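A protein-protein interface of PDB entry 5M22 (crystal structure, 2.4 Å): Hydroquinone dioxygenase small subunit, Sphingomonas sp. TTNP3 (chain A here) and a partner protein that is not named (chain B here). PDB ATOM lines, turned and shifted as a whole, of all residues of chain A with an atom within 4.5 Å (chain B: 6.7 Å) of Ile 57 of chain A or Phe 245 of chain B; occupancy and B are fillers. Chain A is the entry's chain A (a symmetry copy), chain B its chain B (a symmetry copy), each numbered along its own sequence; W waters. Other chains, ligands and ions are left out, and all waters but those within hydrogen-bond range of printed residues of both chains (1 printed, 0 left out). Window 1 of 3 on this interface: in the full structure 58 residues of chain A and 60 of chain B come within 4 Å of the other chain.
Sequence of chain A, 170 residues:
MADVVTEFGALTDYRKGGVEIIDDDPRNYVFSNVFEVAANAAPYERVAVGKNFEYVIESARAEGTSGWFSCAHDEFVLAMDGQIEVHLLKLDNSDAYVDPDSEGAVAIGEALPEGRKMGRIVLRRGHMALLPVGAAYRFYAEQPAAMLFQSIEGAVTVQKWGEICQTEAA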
ATOM      1  N   VAL A  47       8.138  13.169 -11.979  1.00  0.00           N
ATOM      2  CA  VAL A  47       9.582  13.218 -11.811  1.00  0.00           C
ATOM      3  C   VAL A  47       9.860  13.439 -10.347  1.00  0.00           C
ATOM      4  O   VAL A  47       9.266  14.341  -9.715  1.00  0.00           O
ATOM      5  CB  VAL A  47      10.265  14.304 -12.691  1.00  0.00           C
ATOM      6  CG1 VAL A  47      11.771  14.327 -12.488  1.00  0.00           C
ATOM      7  CG2 VAL A  47       9.997  14.051 -14.162  1.00  0.00           C
ATOM      8  N   ALA A  48      10.725  12.583  -9.796  1.00  0.00           N
ATOM      9  CA  ALA A  48      11.072  12.693  -8.399  1.00  0.00           C
ATOM     10  C   ALA A  48      12.089  13.835  -8.237  1.00  0.00           C
ATOM     11  O   ALA A  48      13.041  13.994  -9.043  1.00  0.00           O
ATOM     12  CB  ALA A  48      11.599  11.374  -7.834  1.00  0.00           C
ATOM     13  N   VAL A  49      11.824  14.641  -7.207  1.00  0.00           N
ATOM     14  CA  VAL A  49      12.587  15.815  -6.894  1.00  0.00           C
ATOM     15  C   VAL A  49      13.081  15.686  -5.447  1.00  0.00           C
ATOM     16  O   VAL A  49      13.974  16.421  -5.011  1.00  0.00           O
ATOM     17  CB  VAL A  49      11.719  17.081  -7.094  1.00  0.00           C
ATOM     18  CG1 VAL A  49      11.597  17.417  -8.578  1.00  0.00           C
ATOM     19  CG2 VAL A  49      10.342  16.902  -6.456  1.00  0.00           C
ATOM     20  N   GLY A  50      12.508  14.732  -4.713  1.00  0.00           N
ATOM     21  CA  GLY A  50      12.999  14.368  -3.382  1.00  0.00           C
ATOM     22  C   GLY A  50      12.837  12.887  -3.088  1.00  0.00           C
ATOM     23  O   GLY A  50      11.858  12.270  -3.511  1.00  0.00           O
ATOM     24  N   VAL A  56       9.046   9.448  -1.567  1.00  0.00           N
ATOM     25  CA  VAL A  56       9.408  10.429  -2.572  1.00  0.00           C
ATOM     26  C   VAL A  56       8.431  11.584  -2.625  1.00  0.00           C
ATOM     27  O   VAL A  56       7.271  11.468  -2.206  1.00  0.00           O
ATOM     28  CB  VAL A  56       9.470   9.830  -3.998  1.00  0.00           C
ATOM     29  CG1 VAL A  56      10.678   8.894  -4.175  1.00  0.00           C
ATOM     30  CG2 VAL A  56       8.153   9.140  -4.347  1.00  0.00           C
ATOM     31  N   ILE A  57       8.955  12.708  -3.118  1.00  0.00           N
ATOM     32  CA  ILE A  57       8.169  13.823  -3.600  1.00  0.00           C
ATOM     33  C   ILE A  57       8.392  13.859  -5.097  1.00  0.00           C
ATOM     34  O   ILE A  57       9.517  13.706  -5.555  1.00  0.00           O
ATOM     35  CB  ILE A  57       8.668  15.164  -3.055  1.00  0.00           C
ATOM     36  CG1 ILE A  57       8.625  15.161  -1.522  1.00  0.00           C
ATOM     37  CG2 ILE A  57       7.820  16.283  -3.622  1.00  0.00           C
ATOM     38  CD1 ILE A  57       8.756  16.533  -0.914  1.00  0.00           C
ATOM     39  N   GLU A  58       7.305  14.069  -5.830  1.00  0.00           N
ATOM     40  CA  GLU A  58       7.292  14.083  -7.281  1.00  0.00           C
ATOM     41  C   GLU A  58       6.756  15.393  -7.820  1.00  0.00           C
ATOM     42  O   GLU A  58       5.773  15.938  -7.288  1.00  0.00           O
ATOM     43  CB  GLU A  58       6.417  12.940  -7.796  1.00  0.00           C
ATOM     44  CG  GLU A  58       7.043  11.598  -7.536  1.00  0.00           C
ATOM     45  CD  GLU A  58       6.097  10.441  -7.705  1.00  0.00           C
ATOM     46  OE1 GLU A  58       4.864  10.648  -7.818  1.00  0.00           O
ATOM     47  OE2 GLU A  58       6.618   9.316  -7.777  1.00  0.00           O
ATOM     48  N   SER A  59       7.387  15.901  -8.874  1.00  0.00           N
ATOM     49  CA  SER A  59       6.891  17.102  -9.530  1.00  0.00           C
ATOM     50  C   SER A  59       6.343  16.688 -10.865  1.00  0.00           C
ATOM     51  O   SER A  59       6.894  15.773 -11.493  1.00  0.00           O
ATOM     52  CB  SER A  59       8.005  18.125  -9.723  1.00  0.00           C
ATOM     53  OG  SER A  59       7.537  19.186 -10.538  1.00  0.00           O
ATOM     54  N   MET A 128      -4.129  21.386  -1.082  1.00  0.00           N
ATOM     55  CA  MET A 128      -3.718  19.967  -0.976  1.00  0.00           C
ATOM     56  C   MET A 128      -4.949  19.054  -0.990  1.00  0.00           C
ATOM     57  O   MET A 128      -5.961  19.368  -0.353  1.00  0.00           O
ATOM     58  CB  MET A 128      -2.856  19.719   0.282  1.00  0.00           C
ATOM     59  CG  MET A 128      -2.628  18.257   0.645  1.00  0.00           C
ATOM     60  SD  MET A 128      -1.485  17.914   2.021  1.00  0.00           S
ATOM     61  CE  MET A 128       0.073  18.302   1.239  1.00  0.00           C
ATOM     62  N   LEU A 148       2.695  18.597  -7.035  1.00  0.00           N
ATOM     63  CA  LEU A 148       3.601  17.696  -6.350  1.00  0.00           C
ATOM     64  C   LEU A 148       2.864  16.552  -5.690  1.00  0.00           C
ATOM     65  O   LEU A 148       1.747  16.716  -5.202  1.00  0.00           O
ATOM     66  CB  LEU A 148       4.368  18.435  -5.277  1.00  0.00           C
ATOM     67  CG  LEU A 148       5.300  19.540  -5.711  1.00  0.00           C
ATOM     68  CD1 LEU A 148       5.498  20.396  -4.499  1.00  0.00           C
ATOM     69  CD2 LEU A 148       6.624  18.952  -6.180  1.00  0.00           C
ATOM     70  N   PHE A 149       3.522  15.400  -5.642  1.00  0.00           N
ATOM     71  CA  PHE A 149       2.937  14.221  -5.057  1.00  0.00           C
ATOM     72  C   PHE A 149       3.776  13.844  -3.849  1.00  0.00           C
ATOM     73  O   PHE A 149       4.981  13.794  -3.938  1.00  0.00           O
ATOM     74  CB  PHE A 149       2.886  13.046  -6.089  1.00  0.00           C
ATOM     75  CG  PHE A 149       1.970  13.287  -7.270  1.00  0.00           C
ATOM     76  CD1 PHE A 149       2.440  13.911  -8.433  1.00  0.00           C
ATOM     77  CD2 PHE A 149       0.625  12.904  -7.224  1.00  0.00           C
ATOM     78  CE1 PHE A 149       1.579  14.155  -9.507  1.00  0.00           C
ATOM     79  CE2 PHE A 149      -0.236  13.136  -8.308  1.00  0.00           C
ATOM     80  CZ  PHE A 149       0.247  13.757  -9.448  1.00  0.00           C
ATOM     81  N   GLN A 150       3.126  13.620  -2.715  1.00  0.00           N
ATOM     82  CA  GLN A 150       3.742  12.971  -1.583  1.00  0.00           C
ATOM     83  C   GLN A 150       3.422  11.493  -1.748  1.00  0.00           C
ATOM     84  O   GLN A 150       2.253  11.097  -1.640  1.00  0.00           O
ATOM     85  CB  GLN A 150       3.171  13.518  -0.263  1.00  0.00           C
ATOM     86  CG  GLN A 150       3.656  12.806   1.023  1.00  0.00           C
ATOM     87  CD  GLN A 150       3.154  13.451   2.334  1.00  0.00           C
ATOM     88  OE1 GLN A 150       2.319  14.365   2.317  1.00  0.00           O
ATOM     89  NE2 GLN A 150       3.673  12.984   3.465  1.00  0.00           N
ATOM     90  N   LEU B 221      -3.760  24.832   1.872  1.00  0.00           N
ATOM     91  CA  LEU B 221      -2.564  24.756   2.707  1.00  0.00           C
ATOM     92  C   LEU B 221      -1.772  26.071   2.791  1.00  0.00           C
ATOM     93  O   LEU B 221      -1.304  26.418   3.886  1.00  0.00           O
ATOM     94  CB  LEU B 221      -1.630  23.625   2.277  1.00  0.00           C
ATOM     95  CG  LEU B 221      -0.233  23.603   2.915  1.00  0.00           C
ATOM     96  CD1 LEU B 221      -0.277  23.142   4.364  1.00  0.00           C
ATOM     97  CD2 LEU B 221       0.716  22.714   2.138  1.00  0.00           C
ATOM     98  N   PRO B 234       8.071  23.408  12.445  1.00  0.00           N
ATOM     99  CA  PRO B 234       7.593  22.364  11.550  1.00  0.00           C
ATOM    100  C   PRO B 234       6.441  21.592  12.203  1.00  0.00           C
ATOM    101  O   PRO B 234       6.509  21.199  13.349  1.00  0.00           O
ATOM    102  CB  PRO B 234       8.832  21.479  11.370  1.00  0.00           C
ATOM    103  CG  PRO B 234       9.967  22.433  11.500  1.00  0.00           C
ATOM    104  CD  PRO B 234       9.527  23.293  12.664  1.00  0.00           C
ATOM    105  N   SER B 235       5.356  21.435  11.478  1.00  0.00           N
ATOM    106  CA  SER B 235       4.137  20.958  12.063  1.00  0.00           C
ATOM    107  C   SER B 235       3.445  20.050  11.038  1.00  0.00           C
ATOM    108  O   SER B 235       3.253  20.453   9.910  1.00  0.00           O
ATOM    109  CB  SER B 235       3.319  22.189  12.465  1.00  0.00           C
ATOM    110  OG  SER B 235       1.946  21.927  12.378  1.00  0.00           O
ATOM    111  N   VAL B 236       3.121  18.816  11.418  1.00  0.00           N
ATOM    112  CA  VAL B 236       2.615  17.804  10.464  1.00  0.00           C
ATOM    113  C   VAL B 236       1.247  18.155   9.832  1.00  0.00           C
ATOM    114  O   VAL B 236       0.237  18.298  10.536  1.00  0.00           O
ATOM    115  CB  VAL B 236       2.523  16.371  11.082  1.00  0.00           C
ATOM    116  CG1 VAL B 236       2.126  15.350  10.013  1.00  0.00           C
ATOM    117  CG2 VAL B 236       3.817  15.923  11.758  1.00  0.00           C
ATOM    118  N   CYS B 237       1.204  18.231   8.497  1.00  0.00           N
ATOM    119  CA  CYS B 237      -0.047  18.473   7.766  1.00  0.00           C
ATOM    120  C   CYS B 237      -0.558  17.274   6.932  1.00  0.00           C
ATOM    121  O   CYS B 237      -1.744  17.232   6.616  1.00  0.00           O
ATOM    122  CB  CYS B 237       0.071  19.732   6.891  1.00  0.00           C
ATOM    123  SG  CYS B 237       1.032  19.466   5.394  1.00  0.00           S
ATOM    124  N   SER B 238       0.320  16.342   6.547  1.00  0.00           N
ATOM    125  CA  SER B 238      -0.082  15.103   5.830  1.00  0.00           C
ATOM    126  C   SER B 238       0.912  13.968   6.059  1.00  0.00           C
ATOM    127  O   SER B 238       2.092  14.237   6.244  1.00  0.00           O
ATOM    128  CB  SER B 238      -0.264  15.318   4.325  1.00  0.00           C
ATOM    129  OG  SER B 238       0.748  16.147   3.834  1.00  0.00           O
ATOM    130  N   VAL B 239       0.431  12.718   6.022  1.00  0.00           N
ATOM    131  CA  VAL B 239       1.199  11.560   6.488  1.00  0.00           C
ATOM    132  C   VAL B 239       1.036  10.420   5.485  1.00  0.00           C
ATOM    133  O   VAL B 239      -0.079  10.088   5.134  1.00  0.00           O
ATOM    134  CB  VAL B 239       0.718  11.065   7.896  1.00  0.00           C
ATOM    135  CG1 VAL B 239       1.363   9.746   8.285  1.00  0.00           C
ATOM    136  CG2 VAL B 239       0.951  12.087   8.993  1.00  0.00           C
ATOM    137  N   VAL B 240       2.148   9.835   5.030  1.00  0.00           N
ATOM    138  CA  VAL B 240       2.156   8.550   4.292  1.00  0.00           C
ATOM    139  C   VAL B 240       3.224   7.652   4.941  1.00  0.00           C
ATOM    140  O   VAL B 240       4.415   7.830   4.691  1.00  0.00           O
ATOM    141  CB  VAL B 240       2.513   8.724   2.793  1.00  0.00           C
ATOM    142  CG1 VAL B 240       2.458   7.373   2.087  1.00  0.00           C
ATOM    143  CG2 VAL B 240       1.571   9.697   2.099  1.00  0.00           C
ATOM    144  N   SER B 243       6.594   9.092   6.210  1.00  0.00           N
ATOM    145  CA  SER B 243       6.813  10.297   5.429  1.00  0.00           C
ATOM    146  C   SER B 243       5.938  11.393   5.924  1.00  0.00           C
ATOM    147  O   SER B 243       4.723  11.295   5.761  1.00  0.00           O
ATOM    148  CB  SER B 243       6.433  10.106   3.966  1.00  0.00           C
ATOM    149  OG  SER B 243       6.308  11.385   3.350  1.00  0.00           O
ATOM    150  N   LEU B 244       6.539  12.469   6.436  1.00  0.00           N
ATOM    151  CA  LEU B 244       5.751  13.544   7.078  1.00  0.00           C
ATOM    152  C   LEU B 244       5.979  14.906   6.424  1.00  0.00           C
ATOM    153  O   LEU B 244       7.095  15.364   6.405  1.00  0.00           O
ATOM    154  CB  LEU B 244       6.063  13.618   8.591  1.00  0.00           C
ATOM    155  CG  LEU B 244       6.002  12.315   9.423  1.00  0.00           C
ATOM    156  CD1 LEU B 244       6.523  12.448  10.844  1.00  0.00           C
ATOM    157  CD2 LEU B 244       4.602  11.736   9.448  1.00  0.00           C
ATOM    158  N   PHE B 245       4.922  15.537   5.893  1.00  0.00           N
ATOM    159  CA  PHE B 245       4.995  16.943   5.447  1.00  0.00           C
ATOM    160  C   PHE B 245       4.879  17.906   6.632  1.00  0.00           C
ATOM    161  O   PHE B 245       3.793  18.056   7.216  1.00  0.00           O
ATOM    162  CB  PHE B 245       3.879  17.251   4.444  1.00  0.00           C
ATOM    163  CG  PHE B 245       4.273  17.038   3.007  1.00  0.00           C
ATOM    164  CD1 PHE B 245       5.246  16.077   2.657  1.00  0.00           C
ATOM    165  CD2 PHE B 245       3.668  17.780   1.987  1.00  0.00           C
ATOM    166  CE1 PHE B 245       5.607  15.873   1.323  1.00  0.00           C
ATOM    167  CE2 PHE B 245       4.028  17.582   0.647  1.00  0.00           C
ATOM    168  CZ  PHE B 245       4.989  16.624   0.314  1.00  0.00           C
ATOM    169  N   CYS B 246       5.981  18.561   6.990  1.00  0.00           N
ATOM    170  CA  CYS B 246       5.968  19.490   8.145  1.00  0.00           C
ATOM    171  C   CYS B 246       6.238  20.975   7.764  1.00  0.00           C
ATOM    172  O   CYS B 246       7.320  21.505   8.075  1.00  0.00           O
ATOM    173  CB  CYS B 246       6.956  19.024   9.222  1.00  0.00           C
ATOM    174  SG  CYS B 246       6.940  17.248   9.536  1.00  0.00           S
ATOM    175  N   PRO B 247       5.259  21.641   7.092  1.00  0.00           N
ATOM    176  CA  PRO B 247       5.460  23.041   6.724  1.00  0.00           C
ATOM    177  C   PRO B 247       5.259  23.995   7.917  1.00  0.00           C
ATOM    178  O   PRO B 247       4.624  23.629   8.912  1.00  0.00           O
ATOM    179  CB  PRO B 247       4.403  23.281   5.652  1.00  0.00           C
ATOM    180  CG  PRO B 247       3.289  22.345   6.037  1.00  0.00           C
ATOM    181  CD  PRO B 247       3.921  21.165   6.708  1.00  0.00           C
ATOM    182  N   TRP B 265      14.618  17.169   3.829  1.00  0.00           N
ATOM    183  CA  TRP B 265      14.424  17.956   2.599  1.00  0.00           C
ATOM    184  C   TRP B 265      13.638  19.224   2.899  1.00  0.00           C
ATOM    185  O   TRP B 265      12.733  19.196   3.726  1.00  0.00           O
ATOM    186  CB  TRP B 265      13.649  17.123   1.575  1.00  0.00           C
ATOM    187  CG  TRP B 265      14.469  16.005   1.009  1.00  0.00           C
ATOM    188  CD1 TRP B 265      14.734  14.792   1.595  1.00  0.00           C
ATOM    189  CD2 TRP B 265      15.141  15.993  -0.260  1.00  0.00           C
ATOM    190  NE1 TRP B 265      15.522  14.035   0.761  1.00  0.00           N
ATOM    191  CE2 TRP B 265      15.798  14.752  -0.373  1.00  0.00           C
ATOM    192  CE3 TRP B 265      15.260  16.923  -1.311  1.00  0.00           C
ATOM    193  CZ2 TRP B 265      16.550  14.408  -1.493  1.00  0.00           C
ATOM    194  CZ3 TRP B 265      16.014  16.569  -2.433  1.00  0.00           C
ATOM    195  CH2 TRP B 265      16.648  15.334  -2.508  1.00  0.00           C
ATOM    196  N   LEU B 267      11.503  22.376   0.983  1.00  0.00           N
ATOM    197  CA  LEU B 267      10.896  22.951  -0.231  1.00  0.00           C
ATOM    198  C   LEU B 267      10.371  24.327   0.103  1.00  0.00           C
ATOM    199  O   LEU B 267       9.411  24.454   0.874  1.00  0.00           O
ATOM    200  CB  LEU B 267       9.763  22.083  -0.785  1.00  0.00           C
ATOM    201  CG  LEU B 267       8.855  22.696  -1.859  1.00  0.00           C
ATOM    202  CD1 LEU B 267       9.637  23.059  -3.112  1.00  0.00           C
ATOM    203  CD2 LEU B 267       7.716  21.733  -2.176  1.00  0.00           C
ATOM    204  N   ILE B 296      13.923  23.025  -4.105  1.00  0.00           N
ATOM    205  CA  ILE B 296      13.923  21.902  -3.178  1.00  0.00           C
ATOM    206  C   ILE B 296      15.324  21.377  -3.047  1.00  0.00           C
ATOM    207  O   ILE B 296      15.972  21.097  -4.052  1.00  0.00           O
ATOM    208  CB  ILE B 296      12.890  20.786  -3.557  1.00  0.00           C
ATOM    209  CG1 ILE B 296      13.027  19.586  -2.623  1.00  0.00           C
ATOM    210  CG2 ILE B 296      12.977  20.349  -5.029  1.00  0.00           C
ATOM    211  CD1 ILE B 296      11.987  18.523  -2.893  1.00  0.00           C
ATOM    212  N   LEU B 316       8.373  24.207   3.415  1.00  0.00           N
ATOM    213  CA  LEU B 316       7.985  22.823   3.642  1.00  0.00           C
ATOM    214  C   LEU B 316       9.216  22.003   4.081  1.00  0.00           C
ATOM    215  O   LEU B 316      10.155  21.819   3.277  1.00  0.00           O
ATOM    216  CB  LEU B 316       7.389  22.173   2.379  1.00  0.00           C
ATOM    217  CG  LEU B 316       7.051  20.658   2.498  1.00  0.00           C
ATOM    218  CD1 LEU B 316       5.953  20.390   3.540  1.00  0.00           C
ATOM    219  CD2 LEU B 316       6.695  19.977   1.166  1.00  0.00           C
ATOM    220  N   VAL B 317       9.188  21.525   5.340  1.00  0.00           N
ATOM    221  CA  VAL B 317      10.199  20.626   5.884  1.00  0.00           C
ATOM    222  C   VAL B 317       9.623  19.230   5.693  1.00  0.00           C
ATOM    223  O   VAL B 317       8.488  18.953   6.099  1.00  0.00           O
ATOM    224  CB  VAL B 317      10.479  20.902   7.380  1.00  0.00           C
ATOM    225  CG1 VAL B 317      11.613  20.027   7.876  1.00  0.00           C
ATOM    226  CG2 VAL B 317      10.832  22.373   7.619  1.00  0.00           C
ATOM    227  N   TRP B 318      10.370  18.348   5.046  1.00  0.00           N
ATOM    228  CA  TRP B 318       9.856  17.015   4.757  1.00  0.00           C
ATOM    229  C   TRP B 318      10.750  16.003   5.468  1.00  0.00           C
ATOM    230  O   TRP B 318      11.966  15.999   5.241  1.00  0.00           O
ATOM    231  CB  TRP B 318       9.788  16.775   3.236  1.00  0.00           C
ATOM    232  CG  TRP B 318       9.410  15.354   2.844  1.00  0.00           C
ATOM    233  CD1 TRP B 318       8.368  14.617   3.337  1.00  0.00           C
ATOM    234  CD2 TRP B 318      10.071  14.515   1.880  1.00  0.00           C
ATOM    235  NE1 TRP B 318       8.345  13.372   2.749  1.00  0.00           N
ATOM    236  CE2 TRP B 318       9.377  13.281   1.853  1.00  0.00           C
ATOM    237  CE3 TRP B 318      11.186  14.677   1.048  1.00  0.00           C
ATOM    238  CZ2 TRP B 318       9.764  12.214   1.025  1.00  0.00           C
ATOM    239  CZ3 TRP B 318      11.563  13.620   0.220  1.00  0.00           C
ATOM    240  CH2 TRP B 318      10.850  12.398   0.223  1.00  0.00           C
ATOM    241  N   GLU B 319      10.151  15.181   6.335  1.00  0.00           N
ATOM    242  CA  GLU B 319      10.883  14.221   7.169  1.00  0.00           C
ATOM    243  C   GLU B 319      10.516  12.740   6.912  1.00  0.00           C
ATOM    244  O   GLU B 319       9.351  12.400   6.642  1.00  0.00           O
ATOM    245  CB  GLU B 319      10.648  14.489   8.664  1.00  0.00           C
ATOM    246  CG  GLU B 319      10.902  15.890   9.181  1.00  0.00           C
ATOM    247  CD  GLU B 319      12.373  16.197   9.520  1.00  0.00           C
ATOM    248  OE1 GLU B 319      13.281  15.299   9.513  1.00  0.00           O
ATOM    249  OE2 GLU B 319      12.609  17.387   9.836  1.00  0.00           O
HETATM  250  O   HOH W   1       6.765  10.887   0.566  1.00  0.00           O
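The side-chain sulfur of Met 128 of chain A lies within hydrogen-bond range of the side-chain hydroxyl of Ser 238 of chain B (3.4 Å).
OE1 of Gln 150 of chain A sits at hydrogen-bond distance from OG of Ser 238 of chain B, at 2.8 Å.
The side-chain amide nitrogen (NE2) of Gln 150 of chain A is in hydrogen-bond range of the backbone carbonyl oxygen (O) of Ser 243 of chain B, 3.0 Å away.
Ala 48 of chain A touches none of the printed residues of chain B.
Ile 57 of chain A touches two residues of chain B.
Of the printed residues of chain B, Leu 148 of chain A touches Leu 267.
Of the printed residues of chain B, Gln 150 of chain A touches Ser 238, Val 240, Ser 243 and Phe 245.
Val 239 of chain B touches none of the printed residues of chain A.
Phe 245 of chain B touches three residues of chain A.
Printed residues of chain A within 4 Å of Leu 267 of chain B: Leu 148 (3.5 Å).
Of the printed residues of chain A, Ile 296 of chain B touches Val 49 (3.6 Å).
Among the printed residues, pairs that only touch across the chains: Val 49 of chain A with Trp 265 of chain B, Gln 150 of chain A with Phe 245 of chain B, Leu 148 of chain A with Leu 267 of chain B, Val 49 of chain A with Ile 296 of chain B, Gly 50 of chain A with Trp 318 of chain B, Ile 57 of chain A with Trp 318 of chain B, Met 128 of chain A with Phe 245 of chain B, Val 56 of chain A with Trp 318 of chain B, Gln 150 of chain A with Val 240 of chain B, Gly 50 of chain A with Trp 265 of chain B and Ile 57 of chain A with Phe 245 of chain B.
Water W1 bridges the side-chain hydroxyl (OG) of Ser 243 of chain B (2.9 Å) and the backbone carbonyl oxygen (O) of Val 56 of chain A (2.9 Å).
N of Val 49 of chain A is in hydrogen-bond range of O of Ile 57 of chain A, 3.0 Å away.
The side-chain hydroxyl (OG) of Ser 238 of chain B lies close to the side-chain sulfur (SG) of Cys 237 of chain B (3.7 Å).
N of Phe 245 of chain B lies within hydrogen-bond range of O of Ser 238 of chain B, 3.1 Å away.
The side-chain hydroxyl of Ser 243 of chain B lies within hydrogen-bond range of the indole nitrogen of Trp 318 of chain B (2.9 Å).
O of Trp 265 of chain B lies within hydrogen-bond range of N of Trp 318 of chain B (2.8 Å).
The backbone NH (N) of Leu 267 of chain B sits at hydrogen-bond distance from the backbone carbonyl oxygen (O) of Leu 316 of chain B (2.7 Å).
Printed residues of chain A that touch a printed residue of chain B: Val 49, Gly 50, Val 56, Ile 57, Met 128, Leu 148 and Gln 150.
Hydrophobic or aromatic side chains of chain A within 4 Å of the printed part of chain B: Ile 57, Met 128 and Leu 148.
Of the 20 printed residues of chain B, 8 touch a printed residue of chain A.
Printed residues of chain B that touch a printed residue of chain A: Ser 238, Val 240, Ser 243, Phe 245, Trp 265, Leu 267, Ile 296 and Trp 318.
Hydrophobic or aromatic side chains of chain B that line the printed part of chain A: Val 240, Phe 245, Trp 265, Leu 267, Ile 296 and Trp 318.
Along chain B the printed residues that touch a printed residue of chain A span positions 238 to 318.
Among the printed residues, no Asp or Glu carboxylate lies within 4 Å of a Lys or Arg side-chain nitrogen of the other chain.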
